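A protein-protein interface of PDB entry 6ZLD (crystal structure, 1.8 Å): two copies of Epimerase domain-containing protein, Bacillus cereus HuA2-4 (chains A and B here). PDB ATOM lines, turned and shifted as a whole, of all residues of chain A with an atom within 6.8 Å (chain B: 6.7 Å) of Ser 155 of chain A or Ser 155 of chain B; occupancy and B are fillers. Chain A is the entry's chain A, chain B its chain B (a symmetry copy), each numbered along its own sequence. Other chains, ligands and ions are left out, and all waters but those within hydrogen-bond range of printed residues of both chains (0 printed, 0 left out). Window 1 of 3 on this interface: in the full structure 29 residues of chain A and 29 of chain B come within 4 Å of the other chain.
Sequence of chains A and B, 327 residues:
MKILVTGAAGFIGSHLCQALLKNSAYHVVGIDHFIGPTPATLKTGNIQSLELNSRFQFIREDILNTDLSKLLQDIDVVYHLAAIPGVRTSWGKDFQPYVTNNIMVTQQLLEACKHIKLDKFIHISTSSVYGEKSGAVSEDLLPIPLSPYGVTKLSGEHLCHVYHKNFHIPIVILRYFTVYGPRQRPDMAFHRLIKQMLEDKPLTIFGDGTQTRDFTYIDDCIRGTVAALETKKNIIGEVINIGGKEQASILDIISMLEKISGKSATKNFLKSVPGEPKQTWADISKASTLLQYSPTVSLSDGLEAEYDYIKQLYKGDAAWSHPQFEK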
ATOM      1  N   PHE A  95     -15.825 -29.244 -14.135  1.00  0.00           N
ATOM      2  CA  PHE A  95     -17.212 -28.788 -14.410  1.00  0.00           C
ATOM      3  C   PHE A  95     -17.989 -29.780 -15.292  1.00  0.00           C
ATOM      4  O   PHE A  95     -19.210 -29.986 -15.061  1.00  0.00           O
ATOM      5  CB  PHE A  95     -17.180 -27.394 -15.055  1.00  0.00           C
ATOM      6  CG  PHE A  95     -18.524 -26.769 -15.329  1.00  0.00           C
ATOM      7  CD1 PHE A  95     -19.445 -26.591 -14.307  1.00  0.00           C
ATOM      8  CD2 PHE A  95     -18.873 -26.359 -16.609  1.00  0.00           C
ATOM      9  CE1 PHE A  95     -20.663 -25.968 -14.546  1.00  0.00           C
ATOM     10  CE2 PHE A  95     -20.118 -25.790 -16.862  1.00  0.00           C
ATOM     11  CZ  PHE A  95     -20.992 -25.552 -15.832  1.00  0.00           C
ATOM     12  N   VAL A  99     -22.231 -30.866 -15.591  1.00  0.00           N
ATOM     13  CA  VAL A  99     -23.135 -30.538 -16.714  1.00  0.00           C
ATOM     14  C   VAL A  99     -23.738 -31.850 -17.221  1.00  0.00           C
ATOM     15  O   VAL A  99     -24.958 -31.934 -17.322  1.00  0.00           O
ATOM     16  CB  VAL A  99     -22.385 -29.752 -17.799  1.00  0.00           C
ATOM     17  CG1 VAL A  99     -23.179 -29.670 -19.099  1.00  0.00           C
ATOM     18  CG2 VAL A  99     -22.010 -28.366 -17.290  1.00  0.00           C
ATOM     19  N   ASN A 102     -25.921 -33.563 -14.086  1.00  0.00           N
ATOM     20  CA  ASN A 102     -26.951 -32.716 -13.436  1.00  0.00           C
ATOM     21  C   ASN A 102     -27.898 -32.183 -14.523  1.00  0.00           C
ATOM     22  O   ASN A 102     -29.059 -32.039 -14.227  1.00  0.00           O
ATOM     23  CB  ASN A 102     -26.312 -31.595 -12.602  1.00  0.00           C
ATOM     24  CG  ASN A 102     -25.503 -32.156 -11.450  1.00  0.00           C
ATOM     25  OD1 ASN A 102     -25.482 -33.367 -11.296  1.00  0.00           O
ATOM     26  ND2 ASN A 102     -24.887 -31.313 -10.632  1.00  0.00           N
ATOM     27  N   ILE A 103     -27.392 -31.800 -15.704  1.00  0.00           N
ATOM     28  CA  ILE A 103     -28.255 -31.152 -16.736  1.00  0.00           C
ATOM     29  C   ILE A 103     -28.682 -32.211 -17.756  1.00  0.00           C
ATOM     30  O   ILE A 103     -29.880 -32.449 -17.910  1.00  0.00           O
ATOM     31  CB  ILE A 103     -27.561 -29.938 -17.392  1.00  0.00           C
ATOM     32  CG1 ILE A 103     -27.060 -28.945 -16.335  1.00  0.00           C
ATOM     33  CG2 ILE A 103     -28.490 -29.298 -18.411  1.00  0.00           C
ATOM     34  CD1 ILE A 103     -26.466 -27.672 -16.875  1.00  0.00           C
ATOM     35  N   THR A 106     -30.960 -35.004 -16.290  1.00  0.00           N
ATOM     36  CA  THR A 106     -32.323 -34.542 -15.927  1.00  0.00           C
ATOM     37  C   THR A 106     -33.151 -34.441 -17.206  1.00  0.00           C
ATOM     38  O   THR A 106     -34.297 -34.924 -17.236  1.00  0.00           O
ATOM     39  CB  THR A 106     -32.229 -33.216 -15.182  1.00  0.00           C
ATOM     40  OG1 THR A 106     -31.437 -33.451 -14.017  1.00  0.00           O
ATOM     41  CG2 THR A 106     -33.580 -32.643 -14.826  1.00  0.00           C
ATOM     42  N   HIS A 123     -38.260 -34.237  -7.986  1.00  0.00           N
ATOM     43  CA  HIS A 123     -36.911 -33.817  -8.438  1.00  0.00           C
ATOM     44  C   HIS A 123     -36.173 -33.276  -7.224  1.00  0.00           C
ATOM     45  O   HIS A 123     -36.685 -32.345  -6.574  1.00  0.00           O
ATOM     46  CB  HIS A 123     -36.997 -32.764  -9.536  1.00  0.00           C
ATOM     47  CG  HIS A 123     -35.653 -32.260  -9.930  1.00  0.00           C
ATOM     48  ND1 HIS A 123     -34.885 -32.914 -10.901  1.00  0.00           N
ATOM     49  CD2 HIS A 123     -34.913 -31.235  -9.448  1.00  0.00           C
ATOM     50  CE1 HIS A 123     -33.727 -32.285 -10.998  1.00  0.00           C
ATOM     51  NE2 HIS A 123     -33.714 -31.248 -10.095  1.00  0.00           N
ATOM     52  N   VAL A 129     -28.838 -23.432  -4.818  1.00  0.00           N
ATOM     53  CA  VAL A 129     -29.380 -22.561  -5.898  1.00  0.00           C
ATOM     54  C   VAL A 129     -29.586 -21.135  -5.385  1.00  0.00           C
ATOM     55  O   VAL A 129     -29.539 -20.212  -6.230  1.00  0.00           O
ATOM     56  CB  VAL A 129     -30.656 -23.111  -6.566  1.00  0.00           C
ATOM     57  CG1 VAL A 129     -30.481 -24.551  -7.044  1.00  0.00           C
ATOM     58  CG2 VAL A 129     -31.882 -22.970  -5.684  1.00  0.00           C
ATOM     59  N   TYR A 149     -21.617 -25.762  -9.521  1.00  0.00           N
ATOM     60  CA  TYR A 149     -22.517 -26.840  -9.029  1.00  0.00           C
ATOM     61  C   TYR A 149     -23.946 -26.309  -8.928  1.00  0.00           C
ATOM     62  O   TYR A 149     -24.884 -26.895  -9.511  1.00  0.00           O
ATOM     63  CB  TYR A 149     -22.054 -27.357  -7.662  1.00  0.00           C
ATOM     64  CG  TYR A 149     -23.095 -28.146  -6.902  1.00  0.00           C
ATOM     65  CD1 TYR A 149     -23.641 -29.300  -7.437  1.00  0.00           C
ATOM     66  CD2 TYR A 149     -23.582 -27.729  -5.668  1.00  0.00           C
ATOM     67  CE1 TYR A 149     -24.579 -30.054  -6.745  1.00  0.00           C
ATOM     68  CE2 TYR A 149     -24.511 -28.481  -4.964  1.00  0.00           C
ATOM     69  CZ  TYR A 149     -25.017 -29.659  -5.490  1.00  0.00           C
ATOM     70  OH  TYR A 149     -25.938 -30.419  -4.800  1.00  0.00           O
ATOM     71  N   GLY A 150     -24.094 -25.200  -8.178  1.00  0.00           N
ATOM     72  CA  GLY A 150     -25.406 -24.582  -7.922  1.00  0.00           C
ATOM     73  C   GLY A 150     -26.096 -24.206  -9.233  1.00  0.00           C
ATOM     74  O   GLY A 150     -27.312 -24.398  -9.364  1.00  0.00           O
ATOM     75  N   VAL A 151     -25.325 -23.681 -10.184  1.00  0.00           N
ATOM     76  CA  VAL A 151     -25.824 -23.330 -11.537  1.00  0.00           C
ATOM     77  C   VAL A 151     -26.420 -24.584 -12.213  1.00  0.00           C
ATOM     78  O   VAL A 151     -27.528 -24.470 -12.766  1.00  0.00           O
ATOM     79  CB  VAL A 151     -24.722 -22.699 -12.401  1.00  0.00           C
ATOM     80  CG1 VAL A 151     -25.241 -22.501 -13.807  1.00  0.00           C
ATOM     81  CG2 VAL A 151     -24.208 -21.404 -11.820  1.00  0.00           C
ATOM     82  N   THR A 152     -25.700 -25.698 -12.222  1.00  0.00           N
ATOM     83  CA  THR A 152     -26.153 -26.965 -12.873  1.00  0.00           C
ATOM     84  C   THR A 152     -27.414 -27.516 -12.201  1.00  0.00           C
ATOM     85  O   THR A 152     -28.291 -27.984 -12.928  1.00  0.00           O
ATOM     86  CB  THR A 152     -25.084 -28.064 -12.960  1.00  0.00           C
ATOM     87  OG1 THR A 152     -24.707 -28.503 -11.654  1.00  0.00           O
ATOM     88  CG2 THR A 152     -23.896 -27.620 -13.780  1.00  0.00           C
ATOM     89  N   LYS A 153     -27.533 -27.415 -10.883  1.00  0.00           N
ATOM     90  CA  LYS A 153     -28.740 -27.902 -10.170  1.00  0.00           C
ATOM     91  C   LYS A 153     -29.913 -26.962 -10.501  1.00  0.00           C
ATOM     92  O   LYS A 153     -31.035 -27.446 -10.732  1.00  0.00           O
ATOM     93  CB  LYS A 153     -28.431 -28.011  -8.671  1.00  0.00           C
ATOM     94  CG  LYS A 153     -27.470 -29.142  -8.309  1.00  0.00           C
ATOM     95  CD  LYS A 153     -28.063 -30.539  -8.550  1.00  0.00           C
ATOM     96  CE  LYS A 153     -29.223 -30.876  -7.637  1.00  0.00           C
ATOM     97  NZ  LYS A 153     -29.698 -32.270  -7.840  1.00  0.00           N
ATOM     98  N   LEU A 154     -29.680 -25.654 -10.573  1.00  0.00           N
ATOM     99  CA  LEU A 154     -30.784 -24.729 -10.899  1.00  0.00           C
ATOM    100  C   LEU A 154     -31.202 -25.004 -12.352  1.00  0.00           C
ATOM    101  O   LEU A 154     -32.408 -25.007 -12.630  1.00  0.00           O
ATOM    102  CB  LEU A 154     -30.343 -23.292 -10.655  1.00  0.00           C
ATOM    103  CG  LEU A 154     -31.402 -22.218 -10.835  1.00  0.00           C
ATOM    104  CD1 LEU A 154     -32.631 -22.469  -9.978  1.00  0.00           C
ATOM    105  CD2 LEU A 154     -30.778 -20.860 -10.551  1.00  0.00           C
ATOM    106  N   SER A 155     -30.263 -25.265 -13.267  1.00  0.00           N
ATOM    107  CA  SER A 155     -30.641 -25.644 -14.665  1.00  0.00           C
ATOM    108  C   SER A 155     -31.553 -26.878 -14.635  1.00  0.00           C
ATOM    109  O   SER A 155     -32.506 -26.911 -15.424  1.00  0.00           O
ATOM    110  CB  SER A 155     -29.448 -25.787 -15.604  1.00  0.00           C
ATOM    111  OG  SER A 155     -28.756 -24.535 -15.674  1.00  0.00           O
ATOM    112  N   GLY A 156     -31.322 -27.836 -13.714  1.00  0.00           N
ATOM    113  CA  GLY A 156     -32.171 -29.030 -13.576  1.00  0.00           C
ATOM    114  C   GLY A 156     -33.583 -28.671 -13.165  1.00  0.00           C
ATOM    115  O   GLY A 156     -34.538 -29.185 -13.773  1.00  0.00           O
ATOM    116  N   GLU A 157     -33.724 -27.771 -12.195  1.00  0.00           N
ATOM    117  CA  GLU A 157     -35.028 -27.232 -11.758  1.00  0.00           C
ATOM    118  C   GLU A 157     -35.737 -26.619 -12.967  1.00  0.00           C
ATOM    119  O   GLU A 157     -36.921 -26.969 -13.190  1.00  0.00           O
ATOM    120  CB  GLU A 157     -34.917 -26.199 -10.652  1.00  0.00           C
ATOM    121  CG  GLU A 157     -34.458 -26.745  -9.322  1.00  0.00           C
ATOM    122  CD  GLU A 157     -34.603 -25.720  -8.205  1.00  0.00           C
ATOM    123  OE1 GLU A 157     -35.301 -24.714  -8.438  1.00  0.00           O
ATOM    124  OE2 GLU A 157     -33.980 -25.906  -7.123  1.00  0.00           O
ATOM    125  N   HIS A 158     -35.063 -25.734 -13.704  1.00  0.00           N
ATOM    126  CA  HIS A 158     -35.676 -25.045 -14.880  1.00  0.00           C
ATOM    127  C   HIS A 158     -36.117 -26.062 -15.936  1.00  0.00           C
ATOM    128  O   HIS A 158     -37.219 -25.845 -16.561  1.00  0.00           O
ATOM    129  CB  HIS A 158     -34.720 -24.013 -15.464  1.00  0.00           C
ATOM    130  CG  HIS A 158     -34.367 -22.882 -14.571  1.00  0.00           C
ATOM    131  ND1 HIS A 158     -33.109 -22.283 -14.597  1.00  0.00           N
ATOM    132  CD2 HIS A 158     -35.088 -22.198 -13.668  1.00  0.00           C
ATOM    133  CE1 HIS A 158     -33.102 -21.264 -13.740  1.00  0.00           C
ATOM    134  NE2 HIS A 158     -34.287 -21.210 -13.155  1.00  0.00           N
ATOM    135  N   LEU A 159     -35.351 -27.125 -16.146  1.00  0.00           N
ATOM    136  CA  LEU A 159     -35.759 -28.196 -17.085  1.00  0.00           C
ATOM    137  C   LEU A 159     -37.057 -28.819 -16.565  1.00  0.00           C
ATOM    138  O   LEU A 159     -37.972 -29.060 -17.390  1.00  0.00           O
ATOM    139  CB  LEU A 159     -34.675 -29.262 -17.222  1.00  0.00           C
ATOM    140  CG  LEU A 159     -33.477 -28.886 -18.090  1.00  0.00           C
ATOM    141  CD1 LEU A 159     -32.404 -29.914 -17.924  1.00  0.00           C
ATOM    142  CD2 LEU A 159     -33.857 -28.727 -19.553  1.00  0.00           C
ATOM    143  N   CYS A 160     -37.151 -29.088 -15.259  1.00  0.00           N
ATOM    144  CA  CYS A 160     -38.407 -29.591 -14.615  1.00  0.00           C
ATOM    145  C   CYS A 160     -39.607 -28.687 -14.997  1.00  0.00           C
ATOM    146  O   CYS A 160     -40.621 -29.222 -15.522  1.00  0.00           O
ATOM    147  CB  CYS A 160     -38.236 -29.709 -13.107  1.00  0.00           C
ATOM    148  SG  CYS A 160     -37.297 -31.191 -12.639  1.00  0.00           S
ATOM    149  N   ASN B 102     -23.695 -23.457 -25.378  1.00  0.00           N
ATOM    150  CA  ASN B 102     -24.264 -22.355 -24.563  1.00  0.00           C
ATOM    151  C   ASN B 102     -23.734 -22.414 -23.122  1.00  0.00           C
ATOM    152  O   ASN B 102     -23.624 -21.335 -22.491  1.00  0.00           O
ATOM    153  CB  ASN B 102     -25.792 -22.362 -24.553  1.00  0.00           C
ATOM    154  CG  ASN B 102     -26.349 -22.119 -25.943  1.00  0.00           C
ATOM    155  OD1 ASN B 102     -25.573 -21.886 -26.877  1.00  0.00           O
ATOM    156  ND2 ASN B 102     -27.662 -22.231 -26.114  1.00  0.00           N
ATOM    157  N   ILE B 103     -23.501 -23.617 -22.608  1.00  0.00           N
ATOM    158  CA  ILE B 103     -23.062 -23.797 -21.199  1.00  0.00           C
ATOM    159  C   ILE B 103     -21.556 -24.055 -21.178  1.00  0.00           C
ATOM    160  O   ILE B 103     -20.854 -23.207 -20.563  1.00  0.00           O
ATOM    161  CB  ILE B 103     -23.877 -24.869 -20.432  1.00  0.00           C
ATOM    162  CG1 ILE B 103     -25.369 -24.532 -20.461  1.00  0.00           C
ATOM    163  CG2 ILE B 103     -23.349 -24.972 -19.000  1.00  0.00           C
ATOM    164  CD1 ILE B 103     -26.260 -25.412 -19.614  1.00  0.00           C
ATOM    165  N   THR B 106     -19.427 -21.067 -22.501  1.00  0.00           N
ATOM    166  CA  THR B 106     -19.442 -19.893 -21.607  1.00  0.00           C
ATOM    167  C   THR B 106     -18.478 -20.174 -20.441  1.00  0.00           C
ATOM    168  O   THR B 106     -17.661 -19.308 -20.089  1.00  0.00           O
ATOM    169  CB  THR B 106     -20.884 -19.568 -21.218  1.00  0.00           C
ATOM    170  OG1 THR B 106     -21.626 -19.220 -22.406  1.00  0.00           O
ATOM    171  CG2 THR B 106     -20.976 -18.419 -20.228  1.00  0.00           C
ATOM    172  N   HIS B 123     -21.687 -10.302 -22.067  1.00  0.00           N
ATOM    173  CA  HIS B 123     -22.337 -11.617 -22.303  1.00  0.00           C
ATOM    174  C   HIS B 123     -23.704 -11.382 -22.928  1.00  0.00           C
ATOM    175  O   HIS B 123     -24.546 -10.731 -22.280  1.00  0.00           O
ATOM    176  CB  HIS B 123     -22.452 -12.424 -20.998  1.00  0.00           C
ATOM    177  CG  HIS B 123     -23.060 -13.766 -21.215  1.00  0.00           C
ATOM    178  ND1 HIS B 123     -22.303 -14.834 -21.595  1.00  0.00           N
ATOM    179  CD2 HIS B 123     -24.357 -14.178 -21.196  1.00  0.00           C
ATOM    180  CE1 HIS B 123     -23.062 -15.890 -21.737  1.00  0.00           C
ATOM    181  NE2 HIS B 123     -24.366 -15.511 -21.499  1.00  0.00           N
ATOM    182  N   VAL B 129     -35.048 -16.152 -21.450  1.00  0.00           N
ATOM    183  CA  VAL B 129     -34.834 -16.590 -20.040  1.00  0.00           C
ATOM    184  C   VAL B 129     -36.103 -16.313 -19.208  1.00  0.00           C
ATOM    185  O   VAL B 129     -36.299 -16.986 -18.171  1.00  0.00           O
ATOM    186  CB  VAL B 129     -33.575 -15.958 -19.403  1.00  0.00           C
ATOM    187  CG1 VAL B 129     -32.317 -16.259 -20.222  1.00  0.00           C
ATOM    188  CG2 VAL B 129     -33.715 -14.467 -19.139  1.00  0.00           C
ATOM    189  N   GLY B 150     -33.855 -21.713 -23.655  1.00  0.00           N
ATOM    190  CA  GLY B 150     -33.921 -20.685 -22.605  1.00  0.00           C
ATOM    191  C   GLY B 150     -33.200 -21.096 -21.332  1.00  0.00           C
ATOM    192  O   GLY B 150     -32.533 -20.241 -20.723  1.00  0.00           O
ATOM    193  N   VAL B 151     -33.357 -22.350 -20.916  1.00  0.00           N
ATOM    194  CA  VAL B 151     -32.658 -22.919 -19.730  1.00  0.00           C
ATOM    195  C   VAL B 151     -31.150 -22.780 -19.947  1.00  0.00           C
ATOM    196  O   VAL B 151     -30.466 -22.338 -19.009  1.00  0.00           O
ATOM    197  CB  VAL B 151     -33.034 -24.388 -19.492  1.00  0.00           C
ATOM    198  CG1 VAL B 151     -32.170 -25.002 -18.397  1.00  0.00           C
ATOM    199  CG2 VAL B 151     -34.505 -24.528 -19.161  1.00  0.00           C
ATOM    200  N   THR B 152     -30.642 -23.173 -21.125  1.00  0.00           N
ATOM    201  CA  THR B 152     -29.177 -23.172 -21.370  1.00  0.00           C
ATOM    202  C   THR B 152     -28.673 -21.724 -21.327  1.00  0.00           C
ATOM    203  O   THR B 152     -27.545 -21.511 -20.844  1.00  0.00           O
ATOM    204  CB  THR B 152     -28.737 -23.912 -22.646  1.00  0.00           C
ATOM    205  OG1 THR B 152     -29.255 -23.247 -23.802  1.00  0.00           O
ATOM    206  CG2 THR B 152     -29.141 -25.371 -22.659  1.00  0.00           C
ATOM    207  N   LYS B 153     -29.441 -20.756 -21.836  1.00  0.00           N
ATOM    208  CA  LYS B 153     -28.984 -19.351 -21.872  1.00  0.00           C
ATOM    209  C   LYS B 153     -29.019 -18.793 -20.452  1.00  0.00           C
ATOM    210  O   LYS B 153     -28.145 -18.014 -20.081  1.00  0.00           O
ATOM    211  CB  LYS B 153     -29.834 -18.538 -22.859  1.00  0.00           C
ATOM    212  CG  LYS B 153     -29.585 -18.886 -24.318  1.00  0.00           C
ATOM    213  CD  LYS B 153     -28.238 -18.460 -24.902  1.00  0.00           C
ATOM    214  CE  LYS B 153     -27.987 -16.963 -24.886  1.00  0.00           C
ATOM    215  NZ  LYS B 153     -26.691 -16.639 -25.531  1.00  0.00           N
ATOM    216  N   LEU B 154     -29.990 -19.182 -19.655  1.00  0.00           N
ATOM    217  CA  LEU B 154     -30.041 -18.613 -18.306  1.00  0.00           C
ATOM    218  C   LEU B 154     -28.894 -19.264 -17.511  1.00  0.00           C
ATOM    219  O   LEU B 154     -28.249 -18.591 -16.707  1.00  0.00           O
ATOM    220  CB  LEU B 154     -31.448 -18.814 -17.747  1.00  0.00           C
ATOM    221  CG  LEU B 154     -31.642 -18.426 -16.291  1.00  0.00           C
ATOM    222  CD1 LEU B 154     -31.302 -16.971 -16.040  1.00  0.00           C
ATOM    223  CD2 LEU B 154     -33.052 -18.776 -15.863  1.00  0.00           C
ATOM    224  N   SER B 155     -28.572 -20.521 -17.781  1.00  0.00           N
ATOM    225  CA  SER B 155     -27.384 -21.163 -17.160  1.00  0.00           C
ATOM    226  C   SER B 155     -26.106 -20.340 -17.461  1.00  0.00           C
ATOM    227  O   SER B 155     -25.287 -20.150 -16.533  1.00  0.00           O
ATOM    228  CB  SER B 155     -27.310 -22.591 -17.604  1.00  0.00           C
ATOM    229  OG  SER B 155     -26.308 -23.298 -16.903  1.00  0.00           O
ATOM    230  N   GLY B 156     -25.903 -19.898 -18.706  1.00  0.00           N
ATOM    231  CA  GLY B 156     -24.775 -18.996 -19.039  1.00  0.00           C
ATOM    232  C   GLY B 156     -24.759 -17.713 -18.215  1.00  0.00           C
ATOM    233  O   GLY B 156     -23.665 -17.308 -17.713  1.00  0.00           O
ATOM    234  N   GLU B 157     -25.903 -17.069 -18.048  1.00  0.00           N
ATOM    235  CA  GLU B 157     -25.985 -15.857 -17.200  1.00  0.00           C
ATOM    236  C   GLU B 157     -25.480 -16.239 -15.811  1.00  0.00           C
ATOM    237  O   GLU B 157     -24.704 -15.474 -15.217  1.00  0.00           O
ATOM    238  CB  GLU B 157     -27.414 -15.322 -17.075  1.00  0.00           C
ATOM    239  CG  GLU B 157     -28.020 -14.771 -18.365  1.00  0.00           C
ATOM    240  CD  GLU B 157     -29.284 -13.947 -18.131  1.00  0.00           C
ATOM    241  OE1 GLU B 157     -29.519 -13.585 -16.973  1.00  0.00           O
ATOM    242  OE2 GLU B 157     -30.016 -13.655 -19.099  1.00  0.00           O
ATOM    243  N   HIS B 158     -25.933 -17.380 -15.290  1.00  0.00           N
ATOM    244  CA  HIS B 158     -25.646 -17.747 -13.878  1.00  0.00           C
ATOM    245  C   HIS B 158     -24.142 -17.964 -13.732  1.00  0.00           C
ATOM    246  O   HIS B 158     -23.560 -17.501 -12.703  1.00  0.00           O
ATOM    247  CB  HIS B 158     -26.496 -18.944 -13.397  1.00  0.00           C
ATOM    248  CG  HIS B 158     -27.908 -18.564 -13.144  1.00  0.00           C
ATOM    249  ND1 HIS B 158     -28.962 -19.384 -13.471  1.00  0.00           N
ATOM    250  CD2 HIS B 158     -28.449 -17.437 -12.655  1.00  0.00           C
ATOM    251  CE1 HIS B 158     -30.095 -18.759 -13.195  1.00  0.00           C
ATOM    252  NE2 HIS B 158     -29.817 -17.584 -12.700  1.00  0.00           N
ATOM    253  N   LEU B 159     -23.509 -18.576 -14.736  1.00  0.00           N
ATOM    254  CA  LEU B 159     -22.047 -18.756 -14.778  1.00  0.00           C
ATOM    255  C   LEU B 159     -21.397 -17.373 -14.767  1.00  0.00           C
ATOM    256  O   LEU B 159     -20.458 -17.236 -14.020  1.00  0.00           O
ATOM    257  CB  LEU B 159     -21.638 -19.554 -16.010  1.00  0.00           C
ATOM    258  CG  LEU B 159     -21.962 -21.036 -15.947  1.00  0.00           C
ATOM    259  CD1 LEU B 159     -21.863 -21.709 -17.320  1.00  0.00           C
ATOM    260  CD2 LEU B 159     -21.023 -21.698 -14.947  1.00  0.00           C
ATOM    261  N   CYS B 160     -21.906 -16.372 -15.510  1.00  0.00           N
ATOM    262  CA  CYS B 160     -21.310 -15.006 -15.495  1.00  0.00           C
ATOM    263  C   CYS B 160     -21.323 -14.467 -14.055  1.00  0.00           C
ATOM    264  O   CYS B 160     -20.277 -13.965 -13.592  1.00  0.00           O
ATOM    265  CB  CYS B 160     -22.023 -14.040 -16.438  1.00  0.00           C
ATOM    266  SG  CYS B 160     -21.681 -14.449 -18.163  1.00  0.00           S
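The backbone carbonyl oxygen (O) of Val 151 of chain A lies within hydrogen-bond range of the side-chain hydroxyl (OG) of Ser 155 of chain A, 3.2 Å away.
O of Leu 154 of chain A lies within hydrogen-bond range of ND1 of His 158 of chain A, at 3.4 Å.
The backbone carbonyl oxygen (O) of Leu 154 of chain B lies within hydrogen-bond range of a ring nitrogen (ND1) of His 158 of chain B (3.4 Å).
Ile 103 of chain B touches Phe 95 of chain A.
Leu 159 of chain B touches Phe 95 of chain A.
CD1 of Ile 103 of chain B touches CD1 of Ile 103 of chain A, at 3.6 Å.
Ser 155 of chain B touches Val 151 of chain A.
CG2 of Val 151 of chain A touches CB of His 158 of chain B, 3.7 Å away.
CE1 of His 158 of chain B touches CD2 of Leu 154 of chain A, at 3.4 Å.
Val 151 of chain B touches Ser 155 of chain A.
Val 151 of chain B touches His 158 of chain A.
CE1 of His 158 of chain A touches CD2 of Leu 154 of chain B, 3.3 Å away.
CE1 of His 158 of chain B touches CE1 of His 158 of chain A, at 3.95 Å.
OG of Ser 155 of chain A sits at hydrogen-bond distance from OG of Ser 155 of chain B, 3.0 Å away.
Val 151 of chain A touches His 158 of chain B, and with the chains exchanged His 158 of chain A touches Val 151 of chain B.
Leu 154 of chain A touches His 158 of chain B, and with the chains exchanged His 158 of chain A touches Leu 154 of chain B.
Ser 155 of chain A touches its own counterpart, Ser 155 of chain B.
His 158 of chain B touches its own counterpart, His 158 of chain A.
Positions printed for both chains: 102, 103, 106, 123, 129, 150, 151, 152, 153, 154, 155, 156, 157, 158, 159 and 160.
Printed residues of chain A that touch a printed residue of chain B: Phe 95, Ile 103, Val 151, Leu 154, Ser 155 and His 158.
Hydrophobic or aromatic side chains of chain A within 4 Å of the printed part of chain B: Phe 95, Ile 103, Val 151, Leu 154 and His 158.
Along chain A the printed residues that touch a printed residue of chain B span positions 95 to 158.
Among the printed residues, 11 pairs touch across the chains.
Thr 106 of chain A touches none of the printed residues of chain B.
Printed residues of chain B within 4 Å of Leu 154 of chain A: His 158 (3.4 Å).
Of chain B, only Val 151 (3.5 Å) and Ser 155 (3.0 Å) come within 4 Å of Ser 155 of chain A.
Of the printed residues of chain B, His 158 of chain A touches Val 151, Leu 154 and His 158.
Printed residues of chain A within 4 Å of Ile 103 of chain B: Phe 95 (3.96 Å) and Ile 103 (3.6 Å).
Of chain A, only Val 151 and Ser 155 come within 4 Å of Ser 155 of chain B.
Gly 156 of chain B touches none of the printed residues of chain A.
Printed residues of chain A within 4 Å of His 158 of chain B: Val 151 (3.7 Å), Leu 154 (3.4 Å) and His 158 (3.95 Å).
The nearest printed residue of chain A that does not touch His 158 of chain B is Ser 155 of chain A (5.6 Å).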
